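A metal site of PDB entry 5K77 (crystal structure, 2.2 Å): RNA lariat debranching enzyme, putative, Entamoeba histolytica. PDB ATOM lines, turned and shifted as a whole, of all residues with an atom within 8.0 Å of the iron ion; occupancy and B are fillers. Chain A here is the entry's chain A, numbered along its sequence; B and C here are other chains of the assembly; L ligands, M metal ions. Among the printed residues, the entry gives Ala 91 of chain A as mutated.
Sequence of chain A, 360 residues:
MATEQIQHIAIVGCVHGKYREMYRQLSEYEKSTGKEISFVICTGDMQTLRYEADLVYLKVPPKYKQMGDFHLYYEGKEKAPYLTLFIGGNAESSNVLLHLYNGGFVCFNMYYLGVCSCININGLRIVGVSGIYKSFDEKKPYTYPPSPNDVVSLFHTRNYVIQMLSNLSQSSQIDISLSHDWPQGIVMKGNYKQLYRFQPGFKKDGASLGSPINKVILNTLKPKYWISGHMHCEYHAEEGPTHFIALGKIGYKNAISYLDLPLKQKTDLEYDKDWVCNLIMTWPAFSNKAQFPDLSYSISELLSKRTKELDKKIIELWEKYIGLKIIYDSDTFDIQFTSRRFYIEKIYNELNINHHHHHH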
ATOM      1  N   CYS A  14      12.583  -2.308  -1.679  1.00  0.00           N
ATOM      2  CA  CYS A  14      12.587  -3.056  -2.923  1.00  0.00           C
ATOM      3  C   CYS A  14      12.424  -4.534  -2.654  1.00  0.00           C
ATOM      4  O   CYS A  14      13.148  -5.108  -1.820  1.00  0.00           O
ATOM      5  CB  CYS A  14      13.880  -2.792  -3.699  1.00  0.00           C
ATOM      6  SG  CYS A  14      14.213  -1.078  -4.116  1.00  0.00           S
ATOM      7  N   HIS A  16      12.200  -6.941  -5.496  1.00  0.00           N
ATOM      8  CA  HIS A  16      12.997  -7.562  -6.552  1.00  0.00           C
ATOM      9  C   HIS A  16      12.716  -9.060  -6.654  1.00  0.00           C
ATOM     10  O   HIS A  16      13.622  -9.879  -6.816  1.00  0.00           O
ATOM     11  CB  HIS A  16      14.488  -7.306  -6.352  1.00  0.00           C
ATOM     12  CG  HIS A  16      14.911  -5.906  -6.689  1.00  0.00           C
ATOM     13  ND1 HIS A  16      14.865  -5.405  -7.974  1.00  0.00           N
ATOM     14  CD2 HIS A  16      15.382  -4.905  -5.911  1.00  0.00           C
ATOM     15  CE1 HIS A  16      15.288  -4.161  -7.968  1.00  0.00           C
ATOM     16  NE2 HIS A  16      15.609  -3.828  -6.731  1.00  0.00           N
ATOM     17  N   THR A  43       7.353  -0.106  -1.748  1.00  0.00           N
ATOM     18  CA  THR A  43       7.761   1.076  -2.499  1.00  0.00           C
ATOM     19  C   THR A  43       8.206   0.799  -3.935  1.00  0.00           C
ATOM     20  O   THR A  43       8.601   1.741  -4.628  1.00  0.00           O
ATOM     21  CB  THR A  43       8.888   1.813  -1.758  1.00  0.00           C
ATOM     22  OG1 THR A  43       9.947   0.884  -1.465  1.00  0.00           O
ATOM     23  CG2 THR A  43       8.379   2.419  -0.469  1.00  0.00           C
ATOM     24  N   GLY A  44       8.168  -0.449  -4.403  1.00  0.00           N
ATOM     25  CA  GLY A  44       8.356  -0.678  -5.820  1.00  0.00           C
ATOM     26  C   GLY A  44       9.396  -1.741  -6.107  1.00  0.00           C
ATOM     27  O   GLY A  44       9.903  -2.420  -5.199  1.00  0.00           O
ATOM     28  N   ASP A  45       9.730  -1.874  -7.390  1.00  0.00           N
ATOM     29  CA  ASP A  45      10.582  -2.933  -7.925  1.00  0.00           C
ATOM     30  C   ASP A  45      10.051  -4.304  -7.518  1.00  0.00           C
ATOM     31  O   ASP A  45      10.736  -5.126  -6.901  1.00  0.00           O
ATOM     32  CB  ASP A  45      12.040  -2.737  -7.494  1.00  0.00           C
ATOM     33  CG  ASP A  45      12.725  -1.605  -8.242  1.00  0.00           C
ATOM     34  OD1 ASP A  45      12.131  -1.106  -9.228  1.00  0.00           O
ATOM     35  OD2 ASP A  45      13.846  -1.201  -7.862  1.00  0.00           O
ATOM     36  N   MET A  46       8.798  -4.543  -7.908  1.00  0.00           N
ATOM     37  CA  MET A  46       8.083  -5.750  -7.496  1.00  0.00           C
ATOM     38  C   MET A  46       8.374  -6.934  -8.391  1.00  0.00           C
ATOM     39  O   MET A  46       8.399  -8.073  -7.907  1.00  0.00           O
ATOM     40  CB  MET A  46       6.583  -5.470  -7.468  1.00  0.00           C
ATOM     41  CG  MET A  46       6.197  -4.226  -6.691  1.00  0.00           C
ATOM     42  SD  MET A  46       6.753  -4.279  -4.972  1.00  0.00           S
ATOM     43  CE  MET A  46       5.875  -5.726  -4.371  1.00  0.00           C
ATOM     44  N   GLY A  88       4.800   0.825  -8.595  1.00  0.00           N
ATOM     45  CA  GLY A  88       5.808   0.315  -9.484  1.00  0.00           C
ATOM     46  C   GLY A  88       7.115   1.079  -9.353  1.00  0.00           C
ATOM     47  O   GLY A  88       7.130   2.265  -9.019  1.00  0.00           O
ATOM     48  N   GLY A  89       8.211   0.382  -9.618  1.00  0.00           N
ATOM     49  CA  GLY A  89       9.525   1.004  -9.628  1.00  0.00           C
ATOM     50  C   GLY A  89      10.112   1.034 -11.028  1.00  0.00           C
ATOM     51  O   GLY A  89       9.392   1.293 -12.000  1.00  0.00           O
ATOM     52  N   ASN A  90      11.411   0.767 -11.146  1.00  0.00           N
ATOM     53  CA  ASN A  90      12.071   0.691 -12.433  1.00  0.00           C
ATOM     54  C   ASN A  90      12.333  -0.748 -12.880  1.00  0.00           C
ATOM     55  O   ASN A  90      12.643  -0.959 -14.062  1.00  0.00           O
ATOM     56  CB  ASN A  90      13.401   1.457 -12.402  1.00  0.00           C
ATOM     57  CG  ASN A  90      14.303   0.999 -11.279  1.00  0.00           C
ATOM     58  OD1 ASN A  90      14.084   1.320 -10.110  1.00  0.00           O
ATOM     59  ND2 ASN A  90      15.332   0.238 -11.631  1.00  0.00           N
ATOM     60  N   ALA A  91      12.216  -1.714 -11.988  1.00  0.00           N
ATOM     61  CA  ALA A  91      12.397  -3.131 -12.292  1.00  0.00           C
ATOM     62  C   ALA A  91      11.033  -3.806 -12.135  1.00  0.00           C
ATOM     63  O   ALA A  91      10.686  -4.293 -11.063  1.00  0.00           O
ATOM     64  CB  ALA A  91      13.454  -3.768 -11.389  1.00  0.00           C
ATOM     65  N   GLU A  92      10.256  -3.811 -13.214  1.00  0.00           N
ATOM     66  CA  GLU A  92       8.886  -4.289 -13.171  1.00  0.00           C
ATOM     67  C   GLU A  92       8.569  -5.077 -14.437  1.00  0.00           C
ATOM     68  O   GLU A  92       9.228  -4.929 -15.465  1.00  0.00           O
ATOM     69  CB  GLU A  92       7.887  -3.126 -13.040  1.00  0.00           C
ATOM     70  CG  GLU A  92       8.134  -2.182 -11.873  1.00  0.00           C
ATOM     71  CD  GLU A  92       7.742  -2.771 -10.532  1.00  0.00           C
ATOM     72  OE1 GLU A  92       7.248  -3.924 -10.490  1.00  0.00           O
ATOM     73  OE2 GLU A  92       7.913  -2.088  -9.507  1.00  0.00           O
ATOM     74  N   GLY A 131       7.143   4.558 -10.560  1.00  0.00           N
ATOM     75  CA  GLY A 131       8.207   4.837 -11.512  1.00  0.00           C
ATOM     76  C   GLY A 131       9.356   5.639 -10.938  1.00  0.00           C
ATOM     77  O   GLY A 131       9.399   6.008  -9.761  1.00  0.00           O
ATOM     78  N   ILE A 132      10.323   5.910 -11.817  1.00  0.00           N
ATOM     79  CA  ILE A 132      11.457   6.783 -11.507  1.00  0.00           C
ATOM     80  C   ILE A 132      11.535   7.857 -12.582  1.00  0.00           C
ATOM     81  O   ILE A 132      11.068   7.688 -13.706  1.00  0.00           O
ATOM     82  CB  ILE A 132      12.795   6.024 -11.411  1.00  0.00           C
ATOM     83  CG1 ILE A 132      13.240   5.523 -12.782  1.00  0.00           C
ATOM     84  CG2 ILE A 132      12.676   4.869 -10.424  1.00  0.00           C
ATOM     85  CD1 ILE A 132      14.653   4.959 -12.792  1.00  0.00           C
ATOM     86  N   PHE A 155       8.464   2.583 -17.376  1.00  0.00           N
ATOM     87  CA  PHE A 155       8.564   2.807 -15.941  1.00  0.00           C
ATOM     88  C   PHE A 155       8.992   4.222 -15.576  1.00  0.00           C
ATOM     89  O   PHE A 155       9.237   4.498 -14.404  1.00  0.00           O
ATOM     90  CB  PHE A 155       9.519   1.793 -15.307  1.00  0.00           C
ATOM     91  CG  PHE A 155      10.911   1.830 -15.875  1.00  0.00           C
ATOM     92  CD1 PHE A 155      11.863   2.702 -15.364  1.00  0.00           C
ATOM     93  CD2 PHE A 155      11.274   0.979 -16.902  1.00  0.00           C
ATOM     94  CE1 PHE A 155      13.139   2.732 -15.882  1.00  0.00           C
ATOM     95  CE2 PHE A 155      12.560   1.007 -17.420  1.00  0.00           C
ATOM     96  CZ  PHE A 155      13.492   1.884 -16.910  1.00  0.00           C
ATOM     97  N   HIS A 180       8.945   5.583  -5.559  1.00  0.00           N
ATOM     98  CA  HIS A 180      10.070   4.664  -5.643  1.00  0.00           C
ATOM     99  C   HIS A 180      11.392   5.382  -5.407  1.00  0.00           C
ATOM    100  O   HIS A 180      12.089   5.114  -4.420  1.00  0.00           O
ATOM    101  CB  HIS A 180      10.081   3.935  -6.995  1.00  0.00           C
ATOM    102  CG  HIS A 180      11.085   2.836  -7.057  1.00  0.00           C
ATOM    103  ND1 HIS A 180      11.039   1.741  -6.224  1.00  0.00           N
ATOM    104  CD2 HIS A 180      12.191   2.665  -7.834  1.00  0.00           C
ATOM    105  CE1 HIS A 180      12.056   0.944  -6.483  1.00  0.00           C
ATOM    106  NE2 HIS A 180      12.764   1.473  -7.464  1.00  0.00           N
ATOM    107  N   ASP A 181      11.756   6.306  -6.296  1.00  0.00           N
ATOM    108  CA  ASP A 181      12.930   7.130  -6.036  1.00  0.00           C
ATOM    109  C   ASP A 181      12.574   8.271  -5.086  1.00  0.00           C
ATOM    110  O   ASP A 181      11.402   8.630  -4.920  1.00  0.00           O
ATOM    111  CB  ASP A 181      13.523   7.657  -7.343  1.00  0.00           C
ATOM    112  CG  ASP A 181      12.493   8.316  -8.237  1.00  0.00           C
ATOM    113  OD1 ASP A 181      11.288   8.174  -7.981  1.00  0.00           O
ATOM    114  OD2 ASP A 181      12.909   8.956  -9.229  1.00  0.00           O
ATOM    115  N   GLY A 229      11.986   4.040  -1.807  1.00  0.00           N
ATOM    116  CA  GLY A 229      12.969   2.988  -1.827  1.00  0.00           C
ATOM    117  C   GLY A 229      14.084   3.254  -2.818  1.00  0.00           C
ATOM    118  O   GLY A 229      14.784   4.267  -2.711  1.00  0.00           O
ATOM    119  N   HIS A 230      14.262   2.341  -3.766  1.00  0.00           N
ATOM    120  CA  HIS A 230      15.148   2.508  -4.911  1.00  0.00           C
ATOM    121  C   HIS A 230      16.633   2.526  -4.558  1.00  0.00           C
ATOM    122  O   HIS A 230      17.428   1.863  -5.219  1.00  0.00           O
ATOM    123  CB  HIS A 230      14.783   3.778  -5.686  1.00  0.00           C
ATOM    124  CG  HIS A 230      15.440   3.880  -7.029  1.00  0.00           C
ATOM    125  ND1 HIS A 230      15.571   2.800  -7.881  1.00  0.00           N
ATOM    126  CD2 HIS A 230      16.008   4.936  -7.673  1.00  0.00           C
ATOM    127  CE1 HIS A 230      16.182   3.186  -8.985  1.00  0.00           C
ATOM    128  NE2 HIS A 230      16.459   4.472  -8.888  1.00  0.00           N
ATOM    129  N   MET A 231      17.017   3.270  -3.525  1.00  0.00           N
ATOM    130  CA  MET A 231      18.431   3.516  -3.263  1.00  0.00           C
ATOM    131  C   MET A 231      19.112   2.430  -2.437  1.00  0.00           C
ATOM    132  O   MET A 231      20.316   2.507  -2.221  1.00  0.00           O
ATOM    133  CB  MET A 231      18.608   4.881  -2.583  1.00  0.00           C
ATOM    134  CG  MET A 231      17.964   6.035  -3.345  1.00  0.00           C
ATOM    135  SD  MET A 231      18.632   6.302  -4.996  1.00  0.00           S
ATOM    136  CE  MET A 231      20.173   7.122  -4.606  1.00  0.00           C
ATOM    137  N   HIS A 232      18.358   1.439  -1.960  1.00  0.00           N
ATOM    138  CA  HIS A 232      18.928   0.269  -1.263  1.00  0.00           C
ATOM    139  C   HIS A 232      19.659   0.668   0.013  1.00  0.00           C
ATOM    140  O   HIS A 232      20.736   0.161   0.318  1.00  0.00           O
ATOM    141  CB  HIS A 232      19.852  -0.522  -2.185  1.00  0.00           C
ATOM    142  CG  HIS A 232      19.159  -1.121  -3.365  1.00  0.00           C
ATOM    143  ND1 HIS A 232      19.851  -1.633  -4.444  1.00  0.00           N
ATOM    144  CD2 HIS A 232      17.848  -1.293  -3.639  1.00  0.00           C
ATOM    145  CE1 HIS A 232      18.987  -2.102  -5.336  1.00  0.00           C
ATOM    146  NE2 HIS A 232      17.773  -1.906  -4.875  1.00  0.00           N
ATOM    147  OP3   G B   1      18.470  -1.326 -10.311  1.00  0.00           O
ATOM    148  P     G B   1      17.799  -0.485  -9.130  1.00  0.00           P
ATOM    149  OP1   G B   1      17.885  -1.314  -7.899  1.00  0.00           O
ATOM    150  OP2   G B   1      16.467  -0.014  -9.564  1.00  0.00           O
ATOM    151  O5'   G B   1      18.716   0.806  -8.916  1.00  0.00           O
ATOM    152  C5'   G B   1      19.196   1.159  -7.626  1.00  0.00           C
ATOM    153  C4'   G B   1      20.665   1.506  -7.643  1.00  0.00           C
ATOM    154  O4'   G B   1      20.862   2.749  -8.378  1.00  0.00           O
ATOM    155  C3'   G B   1      21.284   1.730  -6.259  1.00  0.00           C
ATOM    156  O3'   G B   1      22.644   1.314  -6.286  1.00  0.00           O
ATOM    157  C2'   G B   1      21.215   3.239  -6.106  1.00  0.00           C
ATOM    158  O2'   G B   1      22.150   3.782  -5.198  1.00  0.00           O
ATOM    159  C1'   G B   1      21.493   3.701  -7.535  1.00  0.00           C
ATOM    160  N9    G B   1      20.966   5.030  -7.863  1.00  0.00           N
ATOM    161  C8    G B   1      19.707   5.346  -8.311  1.00  0.00           C
ATOM    162  N7    G B   1      19.536   6.627  -8.532  1.00  0.00           N
ATOM    163  C5    G B   1      20.763   7.192  -8.202  1.00  0.00           C
ATOM    164  C6    G B   1      21.195   8.540  -8.230  1.00  0.00           C
ATOM    165  O6    G B   1      20.550   9.546  -8.564  1.00  0.00           O
ATOM    166  N1    G B   1      22.511   8.671  -7.821  1.00  0.00           N
ATOM    167  C2    G B   1      23.322   7.636  -7.426  1.00  0.00           C
ATOM    168  N2    G B   1      24.577   7.958  -7.066  1.00  0.00           N
ATOM    169  N3    G B   1      22.943   6.369  -7.392  1.00  0.00           N
ATOM    170  C4    G B   1      21.652   6.219  -7.793  1.00  0.00           C
ATOM    171  P     U B   2      23.052  -0.187  -5.892  1.00  0.00           P
ATOM    172  OP1   U B   2      22.288  -1.099  -6.790  1.00  0.00           O
ATOM    173  OP2   U B   2      22.834  -0.299  -4.425  1.00  0.00           O
ATOM    174  O5'   U B   2      24.594  -0.266  -6.236  1.00  0.00           O
ATOM    175  P     A C   3      25.112  -3.483 -11.035  1.00  0.00           P
ATOM    176  OP1   A C   3      26.122  -3.898 -10.045  1.00  0.00           O
ATOM    177  OP2   A C   3      24.849  -4.332 -12.218  1.00  0.00           O
ATOM    178  O5'   A C   3      23.719  -3.266 -10.274  1.00  0.00           O
ATOM    179  C5'   A C   3      23.017  -2.026 -10.404  1.00  0.00           C
ATOM    180  C4'   A C   3      21.847  -2.171 -11.364  1.00  0.00           C
ATOM    181  O4'   A C   3      21.181  -3.444 -11.131  1.00  0.00           O
ATOM    182  C3'   A C   3      20.769  -1.110 -11.216  1.00  0.00           C
ATOM    183  O3'   A C   3      20.146  -0.866 -12.473  1.00  0.00           O
ATOM    184  C2'   A C   3      19.797  -1.776 -10.236  1.00  0.00           C
ATOM    185  C1'   A C   3      19.860  -3.227 -10.686  1.00  0.00           C
ATOM    186  N9    A C   3      19.554  -4.184  -9.623  1.00  0.00           N
ATOM    187  C8    A C   3      20.209  -4.312  -8.425  1.00  0.00           C
ATOM    188  N7    A C   3      19.725  -5.271  -7.673  1.00  0.00           N
ATOM    189  C5    A C   3      18.695  -5.804  -8.422  1.00  0.00           C
ATOM    190  C6    A C   3      17.797  -6.858  -8.185  1.00  0.00           C
ATOM    191  N6    A C   3      17.788  -7.587  -7.062  1.00  0.00           N
ATOM    192  N1    A C   3      16.890  -7.145  -9.146  1.00  0.00           N
ATOM    193  C2    A C   3      16.890  -6.413 -10.270  1.00  0.00           C
ATOM    194  N3    A C   3      17.696  -5.401 -10.611  1.00  0.00           N
ATOM    195  C4    A C   3      18.584  -5.147  -9.629  1.00  0.00           C
ATOM    196  P     C C   4      20.519   0.446 -13.307  1.00  0.00           P
ATOM    197  OP1   C C   4      19.839   0.349 -14.631  1.00  0.00           O
ATOM    198  OP2   C C   4      21.985   0.634 -13.253  1.00  0.00           O
ATOM    199  O5'   C C   4      19.841   1.648 -12.498  1.00  0.00           O
ATOM    200  C5'   C C   4      18.430   1.763 -12.391  1.00  0.00           C
ATOM    201  C4'   C C   4      17.928   3.088 -12.905  1.00  0.00           C
ATOM    202  O4'   C C   4      18.478   4.157 -12.101  1.00  0.00           O
ATOM    203  C3'   C C   4      18.302   3.401 -14.354  1.00  0.00           C
ATOM    204  O3'   C C   4      17.232   4.095 -15.003  1.00  0.00           O
ATOM    205  C2'   C C   4      19.499   4.339 -14.207  1.00  0.00           C
ATOM    206  O2'   C C   4      19.701   5.212 -15.293  1.00  0.00           O
ATOM    207  C1'   C C   4      19.125   5.099 -12.935  1.00  0.00           C
ATOM    208  N1    C C   4      20.288   5.657 -12.239  1.00  0.00           N
ATOM    209  C2    C C   4      20.438   7.044 -12.190  1.00  0.00           C
ATOM    210  O2    C C   4      19.565   7.752 -12.732  1.00  0.00           O
ATOM    211  N3    C C   4      21.512   7.573 -11.573  1.00  0.00           N
ATOM    212  C4    C C   4      22.423   6.777 -11.020  1.00  0.00           C
ATOM    213  N4    C C   4      23.466   7.340 -10.418  1.00  0.00           N
ATOM    214  C5    C C   4      22.296   5.358 -11.054  1.00  0.00           C
ATOM    215  C6    C C   4      21.224   4.841 -11.678  1.00  0.00           C
HETATM  216  O1  LIG L   1      15.920   0.069  -6.734  1.00  0.00           O
HETATM  217 FE    FE M   1      14.754   0.701  -8.211  1.00  0.00          FE
HETATM  218 ZN    ZN M   2      15.898  -1.755  -5.930  1.00  0.00          ZN
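The backbone carbonyl oxygen (O) of Asp 45 lies within hydrogen-bond range of the backbone NH (N) of His 16 (2.7 Å).
The side-chain carboxylate of Asp 45 is in hydrogen-bond range of the backbone NH of Ala 91 (2.8 Å).
The side-chain carboxylate (OE2) of Glu 92 sits at hydrogen-bond distance from the backbone NH (N) of Asp 45 (2.8 Å).
O of His 180 is in hydrogen-bond range of N of Gly 229, 2.8 Å away.
ND1 of His 180 sits at hydrogen-bond distance from O of Thr 43, at 2.9 Å.
The side-chain sulfur (SG) of Cys 14 sits close to the backbone NH (N) of His 230 (3.4 Å).
OP1 of G 1 of chain B sits close to NE2 of His 232, at 3.1 Å.
OP3 of G 1 of chain B is bonded to C2' of A 3 of chain C (1.4 Å).
Five residues have an atom within 4 Å of the iron ion: Asp 45, Asn 90, His 180, His 230 and G 1 of chain B.
The iron ion is bound by O1 of the ligand (2.0 Å), OD1 of Asn 90 (2.1 Å), OD2 of Asp 45 (2.1 Å), NE2 of His 180 (2.3 Å), ND1 of His 230 (2.3 Å) and OP2 of G 1 of chain B (2.3 Å).
The iron ion has six donor atoms within binding distance.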
